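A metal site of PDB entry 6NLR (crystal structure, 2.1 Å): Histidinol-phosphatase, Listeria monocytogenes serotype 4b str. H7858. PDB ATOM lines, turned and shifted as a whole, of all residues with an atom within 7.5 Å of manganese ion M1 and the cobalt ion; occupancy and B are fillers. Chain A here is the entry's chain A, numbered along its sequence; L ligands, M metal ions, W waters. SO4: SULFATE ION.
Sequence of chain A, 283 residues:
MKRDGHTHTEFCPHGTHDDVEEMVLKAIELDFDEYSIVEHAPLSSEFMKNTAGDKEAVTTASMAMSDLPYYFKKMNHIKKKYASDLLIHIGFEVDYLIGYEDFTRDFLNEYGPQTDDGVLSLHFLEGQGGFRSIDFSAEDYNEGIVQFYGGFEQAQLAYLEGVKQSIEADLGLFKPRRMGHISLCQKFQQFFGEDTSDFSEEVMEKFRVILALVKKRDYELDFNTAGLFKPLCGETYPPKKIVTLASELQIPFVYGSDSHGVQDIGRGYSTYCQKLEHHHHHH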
ATOM      1  N   HIS A   6      27.269  -8.654  -9.391  1.00  0.00           N
ATOM      2  CA  HIS A   6      26.490  -7.982  -8.309  1.00  0.00           C
ATOM      3  C   HIS A   6      25.034  -8.464  -8.266  1.00  0.00           C
ATOM      4  O   HIS A   6      24.162  -7.880  -8.966  1.00  0.00           O
ATOM      5  CB  HIS A   6      26.661  -6.471  -8.460  1.00  0.00           C
ATOM      6  CG  HIS A   6      26.225  -5.673  -7.278  1.00  0.00           C
ATOM      7  ND1 HIS A   6      26.665  -4.375  -7.080  1.00  0.00           N
ATOM      8  CD2 HIS A   6      25.370  -5.944  -6.273  1.00  0.00           C
ATOM      9  CE1 HIS A   6      26.104  -3.889  -5.990  1.00  0.00           C
ATOM     10  NE2 HIS A   6      25.301  -4.840  -5.470  1.00  0.00           N
ATOM     11  N   THR A   7      24.736  -9.459  -7.421  1.00  0.00           N
ATOM     12  CA  THR A   7      23.356  -9.966  -7.222  1.00  0.00           C
ATOM     13  C   THR A   7      23.081 -10.207  -5.736  1.00  0.00           C
ATOM     14  O   THR A   7      24.042 -10.418  -4.957  1.00  0.00           O
ATOM     15  CB  THR A   7      23.078 -11.247  -8.017  1.00  0.00           C
ATOM     16  OG1 THR A   7      23.764 -12.341  -7.390  1.00  0.00           O
ATOM     17  CG2 THR A   7      23.515 -11.108  -9.458  1.00  0.00           C
ATOM     18  N   HIS A   8      21.803 -10.230  -5.411  1.00  0.00           N
ATOM     19  CA  HIS A   8      21.238 -10.406  -4.053  1.00  0.00           C
ATOM     20  C   HIS A   8      20.326 -11.631  -4.046  1.00  0.00           C
ATOM     21  O   HIS A   8      20.138 -12.248  -5.119  1.00  0.00           O
ATOM     22  CB  HIS A   8      20.577  -9.085  -3.615  1.00  0.00           C
ATOM     23  CG  HIS A   8      21.571  -7.981  -3.476  1.00  0.00           C
ATOM     24  ND1 HIS A   8      22.351  -7.842  -2.332  1.00  0.00           N
ATOM     25  CD2 HIS A   8      21.986  -7.024  -4.329  1.00  0.00           C
ATOM     26  CE1 HIS A   8      23.158  -6.802  -2.489  1.00  0.00           C
ATOM     27  NE2 HIS A   8      22.975  -6.313  -3.729  1.00  0.00           N
ATOM     28  N   HIS A  14      15.135  -6.309   2.154  1.00  0.00           N
ATOM     29  CA  HIS A  14      14.457  -5.305   1.283  1.00  0.00           C
ATOM     30  C   HIS A  14      14.336  -5.806  -0.165  1.00  0.00           C
ATOM     31  O   HIS A  14      13.902  -5.018  -1.017  1.00  0.00           O
ATOM     32  CB  HIS A  14      15.183  -3.955   1.333  1.00  0.00           C
ATOM     33  CG  HIS A  14      16.635  -4.002   0.976  1.00  0.00           C
ATOM     34  ND1 HIS A  14      17.112  -3.840  -0.300  1.00  0.00           N
ATOM     35  CD2 HIS A  14      17.714  -4.149   1.765  1.00  0.00           C
ATOM     36  CE1 HIS A  14      18.430  -3.915  -0.284  1.00  0.00           C
ATOM     37  NE2 HIS A  14      18.822  -4.107   0.971  1.00  0.00           N
ATOM     38  N   VAL A  38      26.569 -11.500  -3.836  1.00  0.00           N
ATOM     39  CA  VAL A  38      27.233 -10.562  -2.912  1.00  0.00           C
ATOM     40  C   VAL A  38      26.144  -9.908  -2.047  1.00  0.00           C
ATOM     41  O   VAL A  38      25.806  -8.725  -2.246  1.00  0.00           O
ATOM     42  CB  VAL A  38      28.139  -9.578  -3.681  1.00  0.00           C
ATOM     43  CG1 VAL A  38      29.411 -10.282  -4.125  1.00  0.00           C
ATOM     44  CG2 VAL A  38      27.442  -8.952  -4.881  1.00  0.00           C
ATOM     45  N   GLU A  39      25.624 -10.693  -1.131  1.00  0.00           N
ATOM     46  CA  GLU A  39      24.522 -10.250  -0.250  1.00  0.00           C
ATOM     47  C   GLU A  39      25.047  -9.140   0.689  1.00  0.00           C
ATOM     48  O   GLU A  39      26.261  -9.146   1.032  1.00  0.00           O
ATOM     49  CB  GLU A  39      23.953 -11.429   0.514  1.00  0.00           C
ATOM     50  CG  GLU A  39      22.643 -11.088   1.176  1.00  0.00           C
ATOM     51  CD  GLU A  39      21.669 -10.439   0.206  1.00  0.00           C
ATOM     52  OE1 GLU A  39      20.981 -11.175  -0.505  1.00  0.00           O
ATOM     53  OE2 GLU A  39      21.628  -9.187   0.179  1.00  0.00           O
ATOM     54  N   HIS A  40      24.166  -8.239   1.108  1.00  0.00           N
ATOM     55  CA  HIS A  40      24.530  -7.188   2.102  1.00  0.00           C
ATOM     56  C   HIS A  40      25.084  -7.822   3.379  1.00  0.00           C
ATOM     57  O   HIS A  40      24.391  -8.661   3.987  1.00  0.00           O
ATOM     58  CB  HIS A  40      23.318  -6.355   2.444  1.00  0.00           C
ATOM     59  CG  HIS A  40      22.809  -5.621   1.262  1.00  0.00           C
ATOM     60  ND1 HIS A  40      23.483  -4.530   0.760  1.00  0.00           N
ATOM     61  CD2 HIS A  40      21.721  -5.808   0.502  1.00  0.00           C
ATOM     62  CE1 HIS A  40      22.815  -4.051  -0.275  1.00  0.00           C
ATOM     63  NE2 HIS A  40      21.734  -4.832  -0.451  1.00  0.00           N
ATOM     64  N   GLU A  93      28.279  -7.725  -0.476  1.00  0.00           N
ATOM     65  CA  GLU A  93      28.298  -6.269  -0.644  1.00  0.00           C
ATOM     66  C   GLU A  93      28.544  -5.711   0.753  1.00  0.00           C
ATOM     67  O   GLU A  93      27.607  -5.747   1.600  1.00  0.00           O
ATOM     68  CB  GLU A  93      27.025  -5.725  -1.275  1.00  0.00           C
ATOM     69  CG  GLU A  93      27.190  -4.262  -1.643  1.00  0.00           C
ATOM     70  CD  GLU A  93      25.975  -3.612  -2.282  1.00  0.00           C
ATOM     71  OE1 GLU A  93      24.959  -4.316  -2.414  1.00  0.00           O
ATOM     72  OE2 GLU A  93      26.061  -2.411  -2.641  1.00  0.00           O
ATOM     73  N   ASP A  95      29.262  -2.818   3.351  1.00  0.00           N
ATOM     74  CA  ASP A  95      29.126  -1.378   3.627  1.00  0.00           C
ATOM     75  C   ASP A  95      30.490  -0.851   4.075  1.00  0.00           C
ATOM     76  O   ASP A  95      31.095  -1.443   4.997  1.00  0.00           O
ATOM     77  CB  ASP A  95      28.053  -1.096   4.684  1.00  0.00           C
ATOM     78  CG  ASP A  95      26.684  -1.028   4.058  1.00  0.00           C
ATOM     79  OD1 ASP A  95      26.308   0.081   3.578  1.00  0.00           O
ATOM     80  OD2 ASP A  95      26.048  -2.082   3.995  1.00  0.00           O
ATOM     81  N   VAL A 119      32.100  -6.738  -3.145  1.00  0.00           N
ATOM     82  CA  VAL A 119      31.902  -5.328  -3.558  1.00  0.00           C
ATOM     83  C   VAL A 119      31.966  -4.510  -2.271  1.00  0.00           C
ATOM     84  O   VAL A 119      31.358  -4.918  -1.256  1.00  0.00           O
ATOM     85  CB  VAL A 119      30.582  -5.176  -4.321  1.00  0.00           C
ATOM     86  CG1 VAL A 119      30.297  -3.741  -4.636  1.00  0.00           C
ATOM     87  CG2 VAL A 119      30.582  -5.996  -5.614  1.00  0.00           C
ATOM     88  N   LEU A 120      32.695  -3.400  -2.296  1.00  0.00           N
ATOM     89  CA  LEU A 120      32.692  -2.437  -1.180  1.00  0.00           C
ATOM     90  C   LEU A 120      31.882  -1.231  -1.624  1.00  0.00           C
ATOM     91  O   LEU A 120      32.264  -0.605  -2.628  1.00  0.00           O
ATOM     92  CB  LEU A 120      34.135  -2.053  -0.826  1.00  0.00           C
ATOM     93  CG  LEU A 120      34.281  -1.088   0.344  1.00  0.00           C
ATOM     94  CD1 LEU A 120      33.859  -1.737   1.639  1.00  0.00           C
ATOM     95  CD2 LEU A 120      35.722  -0.589   0.422  1.00  0.00           C
ATOM     96  N   SER A 121      30.797  -0.956  -0.908  1.00  0.00           N
ATOM     97  CA  SER A 121      29.778   0.042  -1.275  1.00  0.00           C
ATOM     98  C   SER A 121      29.583   1.060  -0.155  1.00  0.00           C
ATOM     99  O   SER A 121      29.500   0.654   1.025  1.00  0.00           O
ATOM    100  CB  SER A 121      28.477  -0.634  -1.591  1.00  0.00           C
ATOM    101  OG  SER A 121      28.592  -1.351  -2.798  1.00  0.00           O
ATOM    102  N   LEU A 122      29.440   2.324  -0.526  1.00  0.00           N
ATOM    103  CA  LEU A 122      29.020   3.403   0.399  1.00  0.00           C
ATOM    104  C   LEU A 122      27.497   3.633   0.257  1.00  0.00           C
ATOM    105  O   LEU A 122      27.052   4.052  -0.846  1.00  0.00           O
ATOM    106  CB  LEU A 122      29.836   4.659   0.085  1.00  0.00           C
ATOM    107  CG  LEU A 122      29.580   5.839   1.011  1.00  0.00           C
ATOM    108  CD1 LEU A 122      30.152   5.562   2.397  1.00  0.00           C
ATOM    109  CD2 LEU A 122      30.147   7.097   0.410  1.00  0.00           C
ATOM    110  N   HIS A 123      26.756   3.451   1.341  1.00  0.00           N
ATOM    111  CA  HIS A 123      25.268   3.613   1.375  1.00  0.00           C
ATOM    112  C   HIS A 123      24.830   4.632   2.430  1.00  0.00           C
ATOM    113  O   HIS A 123      23.657   5.043   2.381  1.00  0.00           O
ATOM    114  CB  HIS A 123      24.555   2.283   1.666  1.00  0.00           C
ATOM    115  CG  HIS A 123      24.766   1.206   0.652  1.00  0.00           C
ATOM    116  ND1 HIS A 123      25.306  -0.020   0.996  1.00  0.00           N
ATOM    117  CD2 HIS A 123      24.526   1.146  -0.672  1.00  0.00           C
ATOM    118  CE1 HIS A 123      25.384  -0.787  -0.079  1.00  0.00           C
ATOM    119  NE2 HIS A 123      24.941  -0.086  -1.113  1.00  0.00           N
ATOM    120  N   ASP A 135      20.375   6.103  -0.346  1.00  0.00           N
ATOM    121  CA  ASP A 135      19.608   5.410  -1.428  1.00  0.00           C
ATOM    122  C   ASP A 135      18.226   4.921  -0.977  1.00  0.00           C
ATOM    123  O   ASP A 135      17.614   4.204  -1.749  1.00  0.00           O
ATOM    124  CB  ASP A 135      20.453   4.262  -2.007  1.00  0.00           C
ATOM    125  CG  ASP A 135      20.794   3.143  -1.036  1.00  0.00           C
ATOM    126  OD1 ASP A 135      20.549   3.306   0.157  1.00  0.00           O
ATOM    127  OD2 ASP A 135      21.302   2.120  -1.492  1.00  0.00           O
ATOM    128  N   GLY A 180      31.587  -0.499  -5.340  1.00  0.00           N
ATOM    129  CA  GLY A 180      30.189  -0.534  -5.739  1.00  0.00           C
ATOM    130  C   GLY A 180      29.658   0.807  -6.239  1.00  0.00           C
ATOM    131  O   GLY A 180      29.988   1.833  -5.643  1.00  0.00           O
ATOM    132  N   HIS A 181      28.855   0.754  -7.299  1.00  0.00           N
ATOM    133  CA  HIS A 181      28.043   1.878  -7.875  1.00  0.00           C
ATOM    134  C   HIS A 181      28.559   3.255  -7.431  1.00  0.00           C
ATOM    135  O   HIS A 181      27.865   3.907  -6.639  1.00  0.00           O
ATOM    136  CB  HIS A 181      26.562   1.676  -7.527  1.00  0.00           C
ATOM    137  CG  HIS A 181      26.287   1.231  -6.120  1.00  0.00           C
ATOM    138  ND1 HIS A 181      26.789   1.926  -5.019  1.00  0.00           N
ATOM    139  CD2 HIS A 181      25.540   0.197  -5.636  1.00  0.00           C
ATOM    140  CE1 HIS A 181      26.350   1.321  -3.899  1.00  0.00           C
ATOM    141  NE2 HIS A 181      25.592   0.253  -4.251  1.00  0.00           N
ATOM    142  N   LEU A 184      26.238   6.765  -6.736  1.00  0.00           N
ATOM    143  CA  LEU A 184      24.940   6.473  -6.064  1.00  0.00           C
ATOM    144  C   LEU A 184      24.264   7.783  -5.613  1.00  0.00           C
ATOM    145  O   LEU A 184      23.057   7.773  -5.398  1.00  0.00           O
ATOM    146  CB  LEU A 184      25.140   5.529  -4.875  1.00  0.00           C
ATOM    147  CG  LEU A 184      23.846   4.961  -4.283  1.00  0.00           C
ATOM    148  CD1 LEU A 184      23.192   3.966  -5.241  1.00  0.00           C
ATOM    149  CD2 LEU A 184      24.118   4.277  -2.949  1.00  0.00           C
ATOM    150  N   ASP A 222      32.399  -1.686 -10.184  1.00  0.00           N
ATOM    151  CA  ASP A 222      31.019  -2.168 -10.403  1.00  0.00           C
ATOM    152  C   ASP A 222      30.404  -1.286 -11.489  1.00  0.00           C
ATOM    153  O   ASP A 222      30.214  -0.076 -11.211  1.00  0.00           O
ATOM    154  CB  ASP A 222      30.301  -2.110  -9.055  1.00  0.00           C
ATOM    155  CG  ASP A 222      28.834  -2.548  -8.965  1.00  0.00           C
ATOM    156  OD1 ASP A 222      28.503  -3.575  -9.570  1.00  0.00           O
ATOM    157  OD2 ASP A 222      28.068  -1.864  -8.220  1.00  0.00           O
ATOM    158  N   ASN A 224      27.238  -0.646 -12.722  1.00  0.00           N
ATOM    159  CA  ASN A 224      25.947  -1.009 -12.094  1.00  0.00           C
ATOM    160  C   ASN A 224      24.777  -0.429 -12.902  1.00  0.00           C
ATOM    161  O   ASN A 224      24.674   0.810 -13.042  1.00  0.00           O
ATOM    162  CB  ASN A 224      26.024  -0.629 -10.627  1.00  0.00           C
ATOM    163  CG  ASN A 224      24.843  -1.104  -9.805  1.00  0.00           C
ATOM    164  OD1 ASN A 224      23.694  -0.987 -10.228  1.00  0.00           O
ATOM    165  ND2 ASN A 224      25.149  -1.640  -8.633  1.00  0.00           N
ATOM    166  N   ALA A 226      21.489  -0.844 -12.230  1.00  0.00           N
ATOM    167  CA  ALA A 226      20.255  -0.680 -11.414  1.00  0.00           C
ATOM    168  C   ALA A 226      19.644   0.710 -11.617  1.00  0.00           C
ATOM    169  O   ALA A 226      18.432   0.816 -11.628  1.00  0.00           O
ATOM    170  CB  ALA A 226      20.551  -0.925  -9.951  1.00  0.00           C
ATOM    171  N   SER A 257      24.136  -6.199 -12.243  1.00  0.00           N
ATOM    172  CA  SER A 257      22.663  -5.994 -12.358  1.00  0.00           C
ATOM    173  C   SER A 257      22.105  -5.423 -11.056  1.00  0.00           C
ATOM    174  O   SER A 257      21.042  -4.814 -11.079  1.00  0.00           O
ATOM    175  CB  SER A 257      21.973  -7.311 -12.678  1.00  0.00           C
ATOM    176  OG  SER A 257      22.144  -8.269 -11.626  1.00  0.00           O
ATOM    177  N   ASP A 258      22.788  -5.649  -9.941  1.00  0.00           N
ATOM    178  CA  ASP A 258      22.242  -5.382  -8.585  1.00  0.00           C
ATOM    179  C   ASP A 258      20.876  -6.069  -8.427  1.00  0.00           C
ATOM    180  O   ASP A 258      19.955  -5.459  -7.849  1.00  0.00           O
ATOM    181  CB  ASP A 258      22.171  -3.880  -8.323  1.00  0.00           C
ATOM    182  CG  ASP A 258      22.606  -3.519  -6.914  1.00  0.00           C
ATOM    183  OD1 ASP A 258      22.480  -4.381  -6.032  1.00  0.00           O
ATOM    184  OD2 ASP A 258      23.117  -2.406  -6.743  1.00  0.00           O
ATOM    185  N   SER A 259      20.719  -7.287  -8.949  1.00  0.00           N
ATOM    186  CA  SER A 259      19.421  -8.004  -9.008  1.00  0.00           C
ATOM    187  C   SER A 259      18.928  -8.325  -7.591  1.00  0.00           C
ATOM    188  O   SER A 259      19.728  -8.873  -6.796  1.00  0.00           O
ATOM    189  CB  SER A 259      19.539  -9.249  -9.851  1.00  0.00           C
ATOM    190  OG  SER A 259      19.638  -8.900 -11.238  1.00  0.00           O
ATOM    191  N   HIS A 260      17.680  -7.973  -7.281  1.00  0.00           N
ATOM    192  CA  HIS A 260      16.992  -8.309  -6.003  1.00  0.00           C
ATOM    193  C   HIS A 260      15.856  -9.310  -6.270  1.00  0.00           C
ATOM    194  O   HIS A 260      15.111  -9.649  -5.299  1.00  0.00           O
ATOM    195  CB  HIS A 260      16.549  -7.015  -5.332  1.00  0.00           C
ATOM    196  CG  HIS A 260      17.691  -6.324  -4.676  1.00  0.00           C
ATOM    197  ND1 HIS A 260      18.676  -5.682  -5.394  1.00  0.00           N
ATOM    198  CD2 HIS A 260      18.021  -6.172  -3.383  1.00  0.00           C
ATOM    199  CE1 HIS A 260      19.554  -5.149  -4.560  1.00  0.00           C
ATOM    200  NE2 HIS A 260      19.197  -5.448  -3.332  1.00  0.00           N
HETATM  201  S   SO4 L   1      21.428  -2.221  -2.923  1.00  0.00           S
HETATM  202  O1  SO4 L   1      22.077  -3.461  -3.308  1.00  0.00           O
HETATM  203  O2  SO4 L   1      20.365  -2.527  -2.012  1.00  0.00           O
HETATM  204  O3  SO4 L   1      20.885  -1.538  -4.086  1.00  0.00           O
HETATM  205  O4  SO4 L   1      22.400  -1.358  -2.278  1.00  0.00           O
HETATM  206 MN    MN M   1      24.530  -1.034  -2.924  1.00  0.00          MN
HETATM  207 CO    CO M   2      23.700  -4.287  -4.182  1.00  0.00          CO
HETATM  208 MN    MN M   3      20.005  -4.364  -1.631  1.00  0.00          MN
HETATM  209  O   HOH W   1      22.966   0.573  -3.513  1.00  0.00           O
HETATM  210  O   HOH W   2      24.048  -2.110  -4.287  1.00  0.00           O
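O1 of the ligand is bound to the cobalt ion, at 2.0 Å. A ring nitrogen (NE2) of His 6 is bound to the cobalt ion, at 2.1 Å. The cobalt ion is bound by OE1 of Glu 93, 2.2 Å away. NE2 of His 8 binds the cobalt ion, at 2.2 Å. Water W2 is bound to the cobalt ion (2.2 Å). The cobalt ion is bound by OD1 of Asp 258, 2.2 Å away. The cobalt ion has six donor atoms within binding distance.
Manganese ion M1 is bound by water W2 (1.8 Å), OE2 of Glu 93 (2.1 Å), NE2 of His 123 (2.1 Å), NE2 of His 181 (2.1 Å), O4 of the ligand (2.2 Å) and water W1 (2.3 Å). Manganese ion M1 has six donor atoms within binding distance.
The side-chain hydroxyl of Ser 121 sits close to the side-chain carboxylate of Glu 93 (2.7 Å). The backbone carbonyl oxygen of Val 38 is in hydrogen-bond range of the backbone NH of Glu 93 (3.2 Å). The backbone NH (N) of Glu 93 is in hydrogen-bond range of the backbone carbonyl oxygen (O) of Glu 39 (2.9 Å). A ring nitrogen (ND1) of His 123 is in hydrogen-bond range of the side-chain carboxylate (OD1) of Asp 95 (2.8 Å). The side-chain amide nitrogen (ND2) of Asn 224 is in hydrogen-bond range of a ring nitrogen (ND1) of His 6, 3.5 Å away. The side-chain carboxylate (OD2) of Asp 222 lies within hydrogen-bond range of a ring nitrogen (ND1) of His 6. The side-chain carboxylate (OE2) of Glu 39 sits at hydrogen-bond distance from a ring nitrogen (ND1) of His 8 (2.9 Å). OD2 of Asp 258 is in hydrogen-bond range of ND2 of Asn 224 (2.9 Å).
Along chain A the residues within 4 Å of manganese ion M1 span positions 93 to 181. The nearest printed residue that does not touch manganese ion M1 is Ser 121 (4.1 Å).
Along chain A the residues within 4 Å of the cobalt ion span positions 6 to 258. The nearest printed residue that does not touch the cobalt ion is His 40 (4.01 Å).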
